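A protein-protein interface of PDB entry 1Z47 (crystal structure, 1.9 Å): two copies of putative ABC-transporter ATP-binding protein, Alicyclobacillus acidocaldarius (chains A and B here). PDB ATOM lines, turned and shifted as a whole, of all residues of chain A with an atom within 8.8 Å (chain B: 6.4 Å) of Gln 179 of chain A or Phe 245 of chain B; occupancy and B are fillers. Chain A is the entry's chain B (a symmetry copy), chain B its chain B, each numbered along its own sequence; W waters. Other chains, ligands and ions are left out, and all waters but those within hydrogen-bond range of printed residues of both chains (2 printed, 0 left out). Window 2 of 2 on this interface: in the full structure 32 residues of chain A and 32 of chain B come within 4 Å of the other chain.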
ATOM      1  N   ILE A 176      31.604 -19.539 -25.209  1.00  0.00           N
ATOM      2  CA  ILE A 176      30.574 -18.657 -24.658  1.00  0.00           C
ATOM      3  C   ILE A 176      29.482 -19.528 -24.024  1.00  0.00           C
ATOM      4  O   ILE A 176      29.296 -20.673 -24.428  1.00  0.00           O
ATOM      5  CB  ILE A 176      29.893 -17.833 -25.779  1.00  0.00           C
ATOM      6  CG1 ILE A 176      29.197 -16.602 -25.203  1.00  0.00           C
ATOM      7  CG2 ILE A 176      28.834 -18.688 -26.472  1.00  0.00           C
ATOM      8  CD1 ILE A 176      30.146 -15.489 -24.854  1.00  0.00           C
ATOM      9  N   ASP A 177      28.768 -18.988 -23.039  1.00  0.00           N
ATOM     10  CA  ASP A 177      27.673 -19.718 -22.406  1.00  0.00           C
ATOM     11  C   ASP A 177      26.538 -19.777 -23.423  1.00  0.00           C
ATOM     12  O   ASP A 177      26.298 -18.806 -24.157  1.00  0.00           O
ATOM     13  CB  ASP A 177      27.169 -18.990 -21.143  1.00  0.00           C
ATOM     14  CG  ASP A 177      27.999 -19.312 -19.894  1.00  0.00           C
ATOM     15  OD1 ASP A 177      28.981 -20.078 -20.005  1.00  0.00           O
ATOM     16  OD2 ASP A 177      27.666 -18.798 -18.799  1.00  0.00           O
ATOM     17  N   THR A 178      25.846 -20.910 -23.448  1.00  0.00           N
ATOM     18  CA  THR A 178      24.719 -21.144 -24.352  1.00  0.00           C
ATOM     19  C   THR A 178      23.698 -19.994 -24.439  1.00  0.00           C
ATOM     20  O   THR A 178      23.271 -19.602 -25.530  1.00  0.00           O
ATOM     21  CB  THR A 178      23.956 -22.425 -23.930  1.00  0.00           C
ATOM     22  OG1 THR A 178      24.859 -23.538 -23.934  1.00  0.00           O
ATOM     23  CG2 THR A 178      22.807 -22.713 -24.879  1.00  0.00           C
ATOM     24  N   GLN A 179      23.302 -19.459 -23.297  1.00  0.00           N
ATOM     25  CA  GLN A 179      22.300 -18.402 -23.292  1.00  0.00           C
ATOM     26  C   GLN A 179      22.786 -17.100 -23.920  1.00  0.00           C
ATOM     27  O   GLN A 179      22.048 -16.431 -24.656  1.00  0.00           O
ATOM     28  CB  GLN A 179      21.837 -18.144 -21.860  1.00  0.00           C
ATOM     29  CG  GLN A 179      20.792 -17.043 -21.735  1.00  0.00           C
ATOM     30  CD  GLN A 179      20.513 -16.690 -20.287  1.00  0.00           C
ATOM     31  OE1 GLN A 179      21.435 -16.465 -19.495  1.00  0.00           O
ATOM     32  NE2 GLN A 179      19.244 -16.628 -19.936  1.00  0.00           N
ATOM     33  N   ILE A 180      24.023 -16.729 -23.622  1.00  0.00           N
ATOM     34  CA  ILE A 180      24.577 -15.499 -24.175  1.00  0.00           C
ATOM     35  C   ILE A 180      24.844 -15.682 -25.672  1.00  0.00           C
ATOM     36  O   ILE A 180      24.635 -14.761 -26.469  1.00  0.00           O
ATOM     37  CB  ILE A 180      25.842 -15.098 -23.399  1.00  0.00           C
ATOM     38  CG1 ILE A 180      25.424 -14.715 -21.966  1.00  0.00           C
ATOM     39  CG2 ILE A 180      26.535 -13.918 -24.074  1.00  0.00           C
ATOM     40  CD1 ILE A 180      26.554 -14.628 -20.973  1.00  0.00           C
ATOM     41  N   ARG A 181      25.267 -16.882 -26.056  1.00  0.00           N
ATOM     42  CA  ARG A 181      25.518 -17.199 -27.466  1.00  0.00           C
ATOM     43  C   ARG A 181      24.218 -16.954 -28.251  1.00  0.00           C
ATOM     44  O   ARG A 181      24.226 -16.396 -29.352  1.00  0.00           O
ATOM     45  CB  ARG A 181      25.928 -18.671 -27.578  1.00  0.00           C
ATOM     46  CG  ARG A 181      26.565 -19.112 -28.888  1.00  0.00           C
ATOM     47  CD  ARG A 181      27.072 -20.559 -28.721  1.00  0.00           C
ATOM     48  NE  ARG A 181      27.310 -21.260 -29.984  1.00  0.00           N
ATOM     49  CZ  ARG A 181      28.255 -20.946 -30.868  1.00  0.00           C
ATOM     50  NH1 ARG A 181      29.076 -19.927 -30.638  1.00  0.00           N
ATOM     51  NH2 ARG A 181      28.375 -21.656 -31.986  1.00  0.00           N
ATOM     52  N   ARG A 182      23.096 -17.372 -27.675  1.00  0.00           N
ATOM     53  CA  ARG A 182      21.812 -17.200 -28.334  1.00  0.00           C
ATOM     54  C   ARG A 182      21.406 -15.735 -28.425  1.00  0.00           C
ATOM     55  O   ARG A 182      20.839 -15.305 -29.441  1.00  0.00           O
ATOM     56  CB  ARG A 182      20.719 -18.014 -27.620  1.00  0.00           C
ATOM     57  CG  ARG A 182      20.887 -19.526 -27.777  1.00  0.00           C
ATOM     58  CD  ARG A 182      19.649 -20.284 -27.330  1.00  0.00           C
ATOM     59  NE  ARG A 182      20.002 -21.607 -26.820  1.00  0.00           N
ATOM     60  CZ  ARG A 182      19.122 -22.528 -26.427  1.00  0.00           C
ATOM     61  NH1 ARG A 182      17.814 -22.275 -26.484  1.00  0.00           N
ATOM     62  NH2 ARG A 182      19.550 -23.704 -25.971  1.00  0.00           N
ATOM     63  N   GLU A 183      21.673 -14.962 -27.376  1.00  0.00           N
ATOM     64  CA  GLU A 183      21.322 -13.544 -27.434  1.00  0.00           C
ATOM     65  C   GLU A 183      22.225 -12.900 -28.468  1.00  0.00           C
ATOM     66  O   GLU A 183      21.793 -12.040 -29.225  1.00  0.00           O
ATOM     67  CB  GLU A 183      21.509 -12.851 -26.075  1.00  0.00           C
ATOM     68  CG  GLU A 183      20.613 -13.388 -24.971  1.00  0.00           C
ATOM     69  CD  GLU A 183      20.898 -12.747 -23.619  1.00  0.00           C
ATOM     70  OE1 GLU A 183      20.275 -13.170 -22.614  1.00  0.00           O
ATOM     71  OE2 GLU A 183      21.742 -11.818 -23.559  1.00  0.00           O
ATOM     72  N   LEU A 184      23.482 -13.321 -28.515  1.00  0.00           N
ATOM     73  CA  LEU A 184      24.397 -12.755 -29.501  1.00  0.00           C
ATOM     74  C   LEU A 184      23.965 -12.972 -30.956  1.00  0.00           C
ATOM     75  O   LEU A 184      23.984 -12.035 -31.775  1.00  0.00           O
ATOM     76  CB  LEU A 184      25.812 -13.322 -29.300  1.00  0.00           C
ATOM     77  CG  LEU A 184      26.644 -12.618 -28.225  1.00  0.00           C
ATOM     78  CD1 LEU A 184      28.035 -13.220 -28.179  1.00  0.00           C
ATOM     79  CD2 LEU A 184      26.707 -11.107 -28.540  1.00  0.00           C
ATOM     80  N   ARG A 185      23.581 -14.197 -31.305  1.00  0.00           N
ATOM     81  CA  ARG A 185      23.191 -14.439 -32.690  1.00  0.00           C
ATOM     82  C   ARG A 185      21.978 -13.597 -33.060  1.00  0.00           C
ATOM     83  O   ARG A 185      21.868 -13.161 -34.192  1.00  0.00           O
ATOM     84  CB  ARG A 185      22.889 -15.918 -32.935  1.00  0.00           C
ATOM     85  CG  ARG A 185      21.694 -16.429 -32.194  1.00  0.00           C
ATOM     86  CD  ARG A 185      21.311 -17.824 -32.692  1.00  0.00           C
ATOM     87  NE  ARG A 185      20.604 -18.600 -31.677  1.00  0.00           N
ATOM     88  CZ  ARG A 185      19.575 -18.159 -30.952  1.00  0.00           C
ATOM     89  NH1 ARG A 185      19.105 -16.927 -31.115  1.00  0.00           N
ATOM     90  NH2 ARG A 185      19.016 -18.957 -30.049  1.00  0.00           N
ATOM     91  N   THR A 186      21.076 -13.358 -32.113  1.00  0.00           N
ATOM     92  CA  THR A 186      19.900 -12.545 -32.402  1.00  0.00           C
ATOM     93  C   THR A 186      20.337 -11.098 -32.642  1.00  0.00           C
ATOM     94  O   THR A 186      19.765 -10.389 -33.470  1.00  0.00           O
ATOM     95  CB  THR A 186      18.872 -12.609 -31.240  1.00  0.00           C
ATOM     96  OG1 THR A 186      18.283 -13.913 -31.212  1.00  0.00           O
ATOM     97  CG2 THR A 186      17.770 -11.585 -31.426  1.00  0.00           C
ATOM     98  N   LEU B  47      23.398 -27.356 -13.575  1.00  0.00           N
ATOM     99  CA  LEU B  47      23.154 -26.323 -14.584  1.00  0.00           C
ATOM    100  C   LEU B  47      23.277 -24.887 -14.070  1.00  0.00           C
ATOM    101  O   LEU B  47      22.572 -24.492 -13.134  1.00  0.00           O
ATOM    102  CB  LEU B  47      21.759 -26.549 -15.173  1.00  0.00           C
ATOM    103  CG  LEU B  47      21.160 -25.482 -16.090  1.00  0.00           C
ATOM    104  CD1 LEU B  47      22.040 -25.289 -17.336  1.00  0.00           C
ATOM    105  CD2 LEU B  47      19.754 -25.909 -16.499  1.00  0.00           C
ATOM    106  N   GLY B  48      24.155 -24.110 -14.697  1.00  0.00           N
ATOM    107  CA  GLY B  48      24.334 -22.723 -14.312  1.00  0.00           C
ATOM    108  C   GLY B  48      25.273 -21.931 -15.222  1.00  0.00           C
ATOM    109  O   GLY B  48      25.964 -22.499 -16.078  1.00  0.00           O
ATOM    110  N   PRO B  49      25.316 -20.603 -15.061  1.00  0.00           N
ATOM    111  CA  PRO B  49      26.192 -19.744 -15.881  1.00  0.00           C
ATOM    112  C   PRO B  49      27.649 -20.054 -15.540  1.00  0.00           C
ATOM    113  O   PRO B  49      27.944 -20.649 -14.503  1.00  0.00           O
ATOM    114  CB  PRO B  49      25.842 -18.332 -15.413  1.00  0.00           C
ATOM    115  CG  PRO B  49      24.428 -18.449 -14.947  1.00  0.00           C
ATOM    116  CD  PRO B  49      24.403 -19.803 -14.228  1.00  0.00           C
ATOM    117  N   THR B 203      27.007 -28.385 -16.846  1.00  0.00           N
ATOM    118  CA  THR B 203      26.542 -27.850 -18.123  1.00  0.00           C
ATOM    119  C   THR B 203      25.963 -26.431 -18.035  1.00  0.00           C
ATOM    120  O   THR B 203      25.371 -26.037 -17.029  1.00  0.00           O
ATOM    121  CB  THR B 203      25.487 -28.792 -18.760  1.00  0.00           C
ATOM    122  OG1 THR B 203      25.152 -28.322 -20.068  1.00  0.00           O
ATOM    123  CG2 THR B 203      24.241 -28.847 -17.923  1.00  0.00           C
ATOM    124  N   HIS B 204      26.155 -25.653 -19.094  1.00  0.00           N
ATOM    125  CA  HIS B 204      25.600 -24.309 -19.137  1.00  0.00           C
ATOM    126  C   HIS B 204      24.497 -24.273 -20.201  1.00  0.00           C
ATOM    127  O   HIS B 204      23.962 -23.205 -20.536  1.00  0.00           O
ATOM    128  CB  HIS B 204      26.704 -23.279 -19.436  1.00  0.00           C
ATOM    129  CG  HIS B 204      27.504 -23.580 -20.672  1.00  0.00           C
ATOM    130  ND1 HIS B 204      26.971 -23.511 -21.941  1.00  0.00           N
ATOM    131  CD2 HIS B 204      28.803 -23.937 -20.830  1.00  0.00           C
ATOM    132  CE1 HIS B 204      27.904 -23.813 -22.828  1.00  0.00           C
ATOM    133  NE2 HIS B 204      29.026 -24.074 -22.179  1.00  0.00           N
ATOM    134  N   ASP B 205      24.136 -25.461 -20.693  1.00  0.00           N
ATOM    135  CA  ASP B 205      23.119 -25.650 -21.742  1.00  0.00           C
ATOM    136  C   ASP B 205      21.834 -26.259 -21.154  1.00  0.00           C
ATOM    137  O   ASP B 205      21.758 -27.461 -20.912  1.00  0.00           O
ATOM    138  CB  ASP B 205      23.663 -26.591 -22.826  1.00  0.00           C
ATOM    139  CG  ASP B 205      22.721 -26.722 -24.019  1.00  0.00           C
ATOM    140  OD1 ASP B 205      21.515 -26.393 -23.886  1.00  0.00           O
ATOM    141  OD2 ASP B 205      23.198 -27.156 -25.095  1.00  0.00           O
ATOM    142  N   GLN B 206      20.810 -25.439 -20.955  1.00  0.00           N
ATOM    143  CA  GLN B 206      19.599 -25.958 -20.351  1.00  0.00           C
ATOM    144  C   GLN B 206      18.953 -27.078 -21.163  1.00  0.00           C
ATOM    145  O   GLN B 206      18.373 -27.997 -20.591  1.00  0.00           O
ATOM    146  CB  GLN B 206      18.609 -24.813 -20.087  1.00  0.00           C
ATOM    147  CG  GLN B 206      18.167 -24.002 -21.313  1.00  0.00           C
ATOM    148  CD  GLN B 206      17.100 -24.702 -22.135  1.00  0.00           C
ATOM    149  OE1 GLN B 206      16.189 -25.341 -21.591  1.00  0.00           O
ATOM    150  NE2 GLN B 206      17.183 -24.559 -23.448  1.00  0.00           N
ATOM    151  N   VAL B 218      19.884 -26.142 -10.446  1.00  0.00           N
ATOM    152  CA  VAL B 218      20.159 -24.839 -11.042  1.00  0.00           C
ATOM    153  C   VAL B 218      20.975 -23.978 -10.069  1.00  0.00           C
ATOM    154  O   VAL B 218      20.580 -23.729  -8.914  1.00  0.00           O
ATOM    155  CB  VAL B 218      18.838 -24.130 -11.424  1.00  0.00           C
ATOM    156  CG1 VAL B 218      19.105 -22.945 -12.367  1.00  0.00           C
ATOM    157  CG2 VAL B 218      17.893 -25.123 -12.058  1.00  0.00           C
ATOM    158  N   LEU B 219      22.141 -23.547 -10.536  1.00  0.00           N
ATOM    159  CA  LEU B 219      23.033 -22.739  -9.744  1.00  0.00           C
ATOM    160  C   LEU B 219      23.068 -21.304 -10.255  1.00  0.00           C
ATOM    161  O   LEU B 219      22.980 -21.044 -11.460  1.00  0.00           O
ATOM    162  CB  LEU B 219      24.451 -23.314  -9.795  1.00  0.00           C
ATOM    163  CG  LEU B 219      24.707 -24.589  -8.991  1.00  0.00           C
ATOM    164  CD1 LEU B 219      24.539 -24.298  -7.497  1.00  0.00           C
ATOM    165  CD2 LEU B 219      23.739 -25.666  -9.442  1.00  0.00           C
ATOM    166  N   LEU B 240      12.631 -16.185 -10.730  1.00  0.00           N
ATOM    167  CA  LEU B 240      12.677 -15.572 -12.035  1.00  0.00           C
ATOM    168  C   LEU B 240      13.906 -16.110 -12.770  1.00  0.00           C
ATOM    169  O   LEU B 240      13.865 -16.315 -13.990  1.00  0.00           O
ATOM    170  CB  LEU B 240      12.762 -14.049 -11.897  1.00  0.00           C
ATOM    171  CG  LEU B 240      13.045 -13.258 -13.174  1.00  0.00           C
ATOM    172  CD1 LEU B 240      11.929 -13.457 -14.209  1.00  0.00           C
ATOM    173  CD2 LEU B 240      13.140 -11.770 -12.794  1.00  0.00           C
ATOM    174  N   PHE B 241      14.994 -16.339 -12.034  1.00  0.00           N
ATOM    175  CA  PHE B 241      16.204 -16.852 -12.682  1.00  0.00           C
ATOM    176  C   PHE B 241      15.944 -18.206 -13.341  1.00  0.00           C
ATOM    177  O   PHE B 241      16.344 -18.414 -14.491  1.00  0.00           O
ATOM    178  CB  PHE B 241      17.395 -17.016 -11.714  1.00  0.00           C
ATOM    179  CG  PHE B 241      18.644 -17.482 -12.407  1.00  0.00           C
ATOM    180  CD1 PHE B 241      19.379 -16.599 -13.196  1.00  0.00           C
ATOM    181  CD2 PHE B 241      19.023 -18.823 -12.373  1.00  0.00           C
ATOM    182  CE1 PHE B 241      20.467 -17.036 -13.949  1.00  0.00           C
ATOM    183  CE2 PHE B 241      20.128 -19.283 -13.133  1.00  0.00           C
ATOM    184  CZ  PHE B 241      20.841 -18.392 -13.916  1.00  0.00           C
ATOM    185  N   VAL B 242      15.295 -19.124 -12.619  1.00  0.00           N
ATOM    186  CA  VAL B 242      14.994 -20.444 -13.186  1.00  0.00           C
ATOM    187  C   VAL B 242      14.072 -20.264 -14.386  1.00  0.00           C
ATOM    188  O   VAL B 242      14.268 -20.864 -15.442  1.00  0.00           O
ATOM    189  CB  VAL B 242      14.296 -21.411 -12.159  1.00  0.00           C
ATOM    190  CG1 VAL B 242      13.994 -22.760 -12.834  1.00  0.00           C
ATOM    191  CG2 VAL B 242      15.197 -21.636 -10.945  1.00  0.00           C
ATOM    192  N   ALA B 243      13.087 -19.385 -14.239  1.00  0.00           N
ATOM    193  CA  ALA B 243      12.147 -19.134 -15.314  1.00  0.00           C
ATOM    194  C   ALA B 243      12.812 -18.588 -16.576  1.00  0.00           C
ATOM    195  O   ALA B 243      12.413 -18.911 -17.694  1.00  0.00           O
ATOM    196  CB  ALA B 243      11.043 -18.172 -14.822  1.00  0.00           C
ATOM    197  N   SER B 244      13.832 -17.761 -16.391  1.00  0.00           N
ATOM    198  CA  SER B 244      14.534 -17.153 -17.507  1.00  0.00           C
ATOM    199  C   SER B 244      15.724 -17.973 -17.999  1.00  0.00           C
ATOM    200  O   SER B 244      16.234 -17.721 -19.077  1.00  0.00           O
ATOM    201  CB  SER B 244      15.033 -15.768 -17.087  1.00  0.00           C
ATOM    202  OG  SER B 244      14.017 -15.094 -16.392  1.00  0.00           O
ATOM    203  N   PHE B 245      16.169 -18.947 -17.217  1.00  0.00           N
ATOM    204  CA  PHE B 245      17.331 -19.742 -17.618  1.00  0.00           C
ATOM    205  C   PHE B 245      16.969 -21.105 -18.229  1.00  0.00           C
ATOM    206  O   PHE B 245      17.761 -21.660 -18.984  1.00  0.00           O
ATOM    207  CB  PHE B 245      18.271 -19.934 -16.414  1.00  0.00           C
ATOM    208  CG  PHE B 245      19.687 -20.289 -16.788  1.00  0.00           C
ATOM    209  CD1 PHE B 245      20.504 -19.372 -17.452  1.00  0.00           C
ATOM    210  CD2 PHE B 245      20.210 -21.544 -16.479  1.00  0.00           C
ATOM    211  CE1 PHE B 245      21.828 -19.698 -17.804  1.00  0.00           C
ATOM    212  CE2 PHE B 245      21.530 -21.875 -16.831  1.00  0.00           C
ATOM    213  CZ  PHE B 245      22.336 -20.946 -17.495  1.00  0.00           C
ATOM    214  N   ILE B 246      15.792 -21.637 -17.900  1.00  0.00           N
ATOM    215  CA  ILE B 246      15.328 -22.933 -18.438  1.00  0.00           C
ATOM    216  C   ILE B 246      14.300 -22.648 -19.531  1.00  0.00           C
ATOM    217  O   ILE B 246      13.417 -21.794 -19.353  1.00  0.00           O
ATOM    218  CB  ILE B 246      14.621 -23.791 -17.360  1.00  0.00           C
ATOM    219  CG1 ILE B 246      15.531 -23.991 -16.155  1.00  0.00           C
ATOM    220  CG2 ILE B 246      14.204 -25.140 -17.948  1.00  0.00           C
ATOM    221  CD1 ILE B 246      16.884 -24.447 -16.505  1.00  0.00           C
ATOM    222  N   GLY B 247      14.407 -23.352 -20.653  1.00  0.00           N
ATOM    223  CA  GLY B 247      13.481 -23.134 -21.752  1.00  0.00           C
ATOM    224  C   GLY B 247      13.770 -21.764 -22.332  1.00  0.00           C
ATOM    225  O   GLY B 247      14.751 -21.119 -21.967  1.00  0.00           O
ATOM    226  N   SER B 249      12.324 -17.782 -23.299  1.00  0.00           N
ATOM    227  CA  SER B 249      11.354 -16.843 -22.745  1.00  0.00           C
ATOM    228  C   SER B 249      11.477 -15.415 -23.206  1.00  0.00           C
ATOM    229  O   SER B 249      12.520 -14.981 -23.685  1.00  0.00           O
ATOM    230  CB  SER B 249      11.413 -16.868 -21.206  1.00  0.00           C
ATOM    231  OG  SER B 249      12.735 -16.637 -20.727  1.00  0.00           O
HETATM  232  O   HOH W   1      15.891 -24.984 -26.640  1.00  0.00           O
HETATM  233  O   HOH W   2      24.031 -20.508 -20.680  1.00  0.00           O
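Water W2 lies within hydrogen-bond range of the backbone carbonyl oxygen of His 204 of chain B (2.7 Å), the backbone NH of Gln 179 of chain A (2.9 Å) and the backbone NH of Thr 178 of chain A (3.3 Å).
Water W1 bridges NH1 of Arg 182 of chain A and NE2 of Gln 206 of chain B.
No position is printed for both chains.
Gln 179 of chain A touches two residues of chain B.
Phe 245 of chain B touches just one residue of chain A: Gln 179 (3.7 Å).
Gly 48 of chain B touches none of the printed residues of chain A.
Ser 244 of chain B touches one residue of chain A.
Of the printed residues of chain B, Asp 177 of chain A touches Pro 49 and His 204.
Of the printed residues of chain A, Pro 49 of chain B touches Asp 177 (3.4 Å).
The nearest residue of chain A that does not touch Phe 245 of chain B is Asp 177 of chain A (5.9 Å).
Of the 18 printed residues of chain B, 6 touch a printed residue of chain A.
Hydrophobic or aromatic side chains of chain B that line the printed part of chain A: Pro 49, His 204 and Phe 245.
OG1 of Thr 178 of chain A sits at hydrogen-bond distance from ND1 of His 204 of chain B (2.9 Å).
OD1 of Asp 205 of chain B lies within salt-bridge range of NH2 of Arg 182 of chain A (3.9 Å).
O of Ser 244 of chain B sits at hydrogen-bond distance from NE2 of Gln 179 of chain A (3.3 Å).
Among the printed residues, pairs that only touch across the chains: Ile 176 of chain A with His 204 of chain B, Asp 177 of chain A with Pro 49 of chain B, Asp 177 of chain A with His 204 of chain B, Thr 178 of chain A with Asp 205 of chain B, Gln 179 of chain A with Phe 245 of chain B and Arg 182 of chain A with Gln 206 of chain B.
The side-chain hydroxyl (OG1) of Thr 186 of chain A sits at hydrogen-bond distance from the backbone carbonyl oxygen (O) of Arg 182 of chain A.
N of Gly 247 of chain B sits at hydrogen-bond distance from OE1 of Gln 206 of chain B (2.8 Å).
The backbone carbonyl oxygen (O) of Arg 182 of chain A is in hydrogen-bond range of the guanidinium group (NH1) of Arg 185 of chain A (2.9 Å).
The side-chain hydroxyl of Thr 203 of chain B sits at hydrogen-bond distance from the backbone NH of Asp 205 of chain B, 3.1 Å away.
The backbone carbonyl oxygen of Leu 240 of chain B is in hydrogen-bond range of the side-chain hydroxyl of Ser 244 of chain B (2.7 Å).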
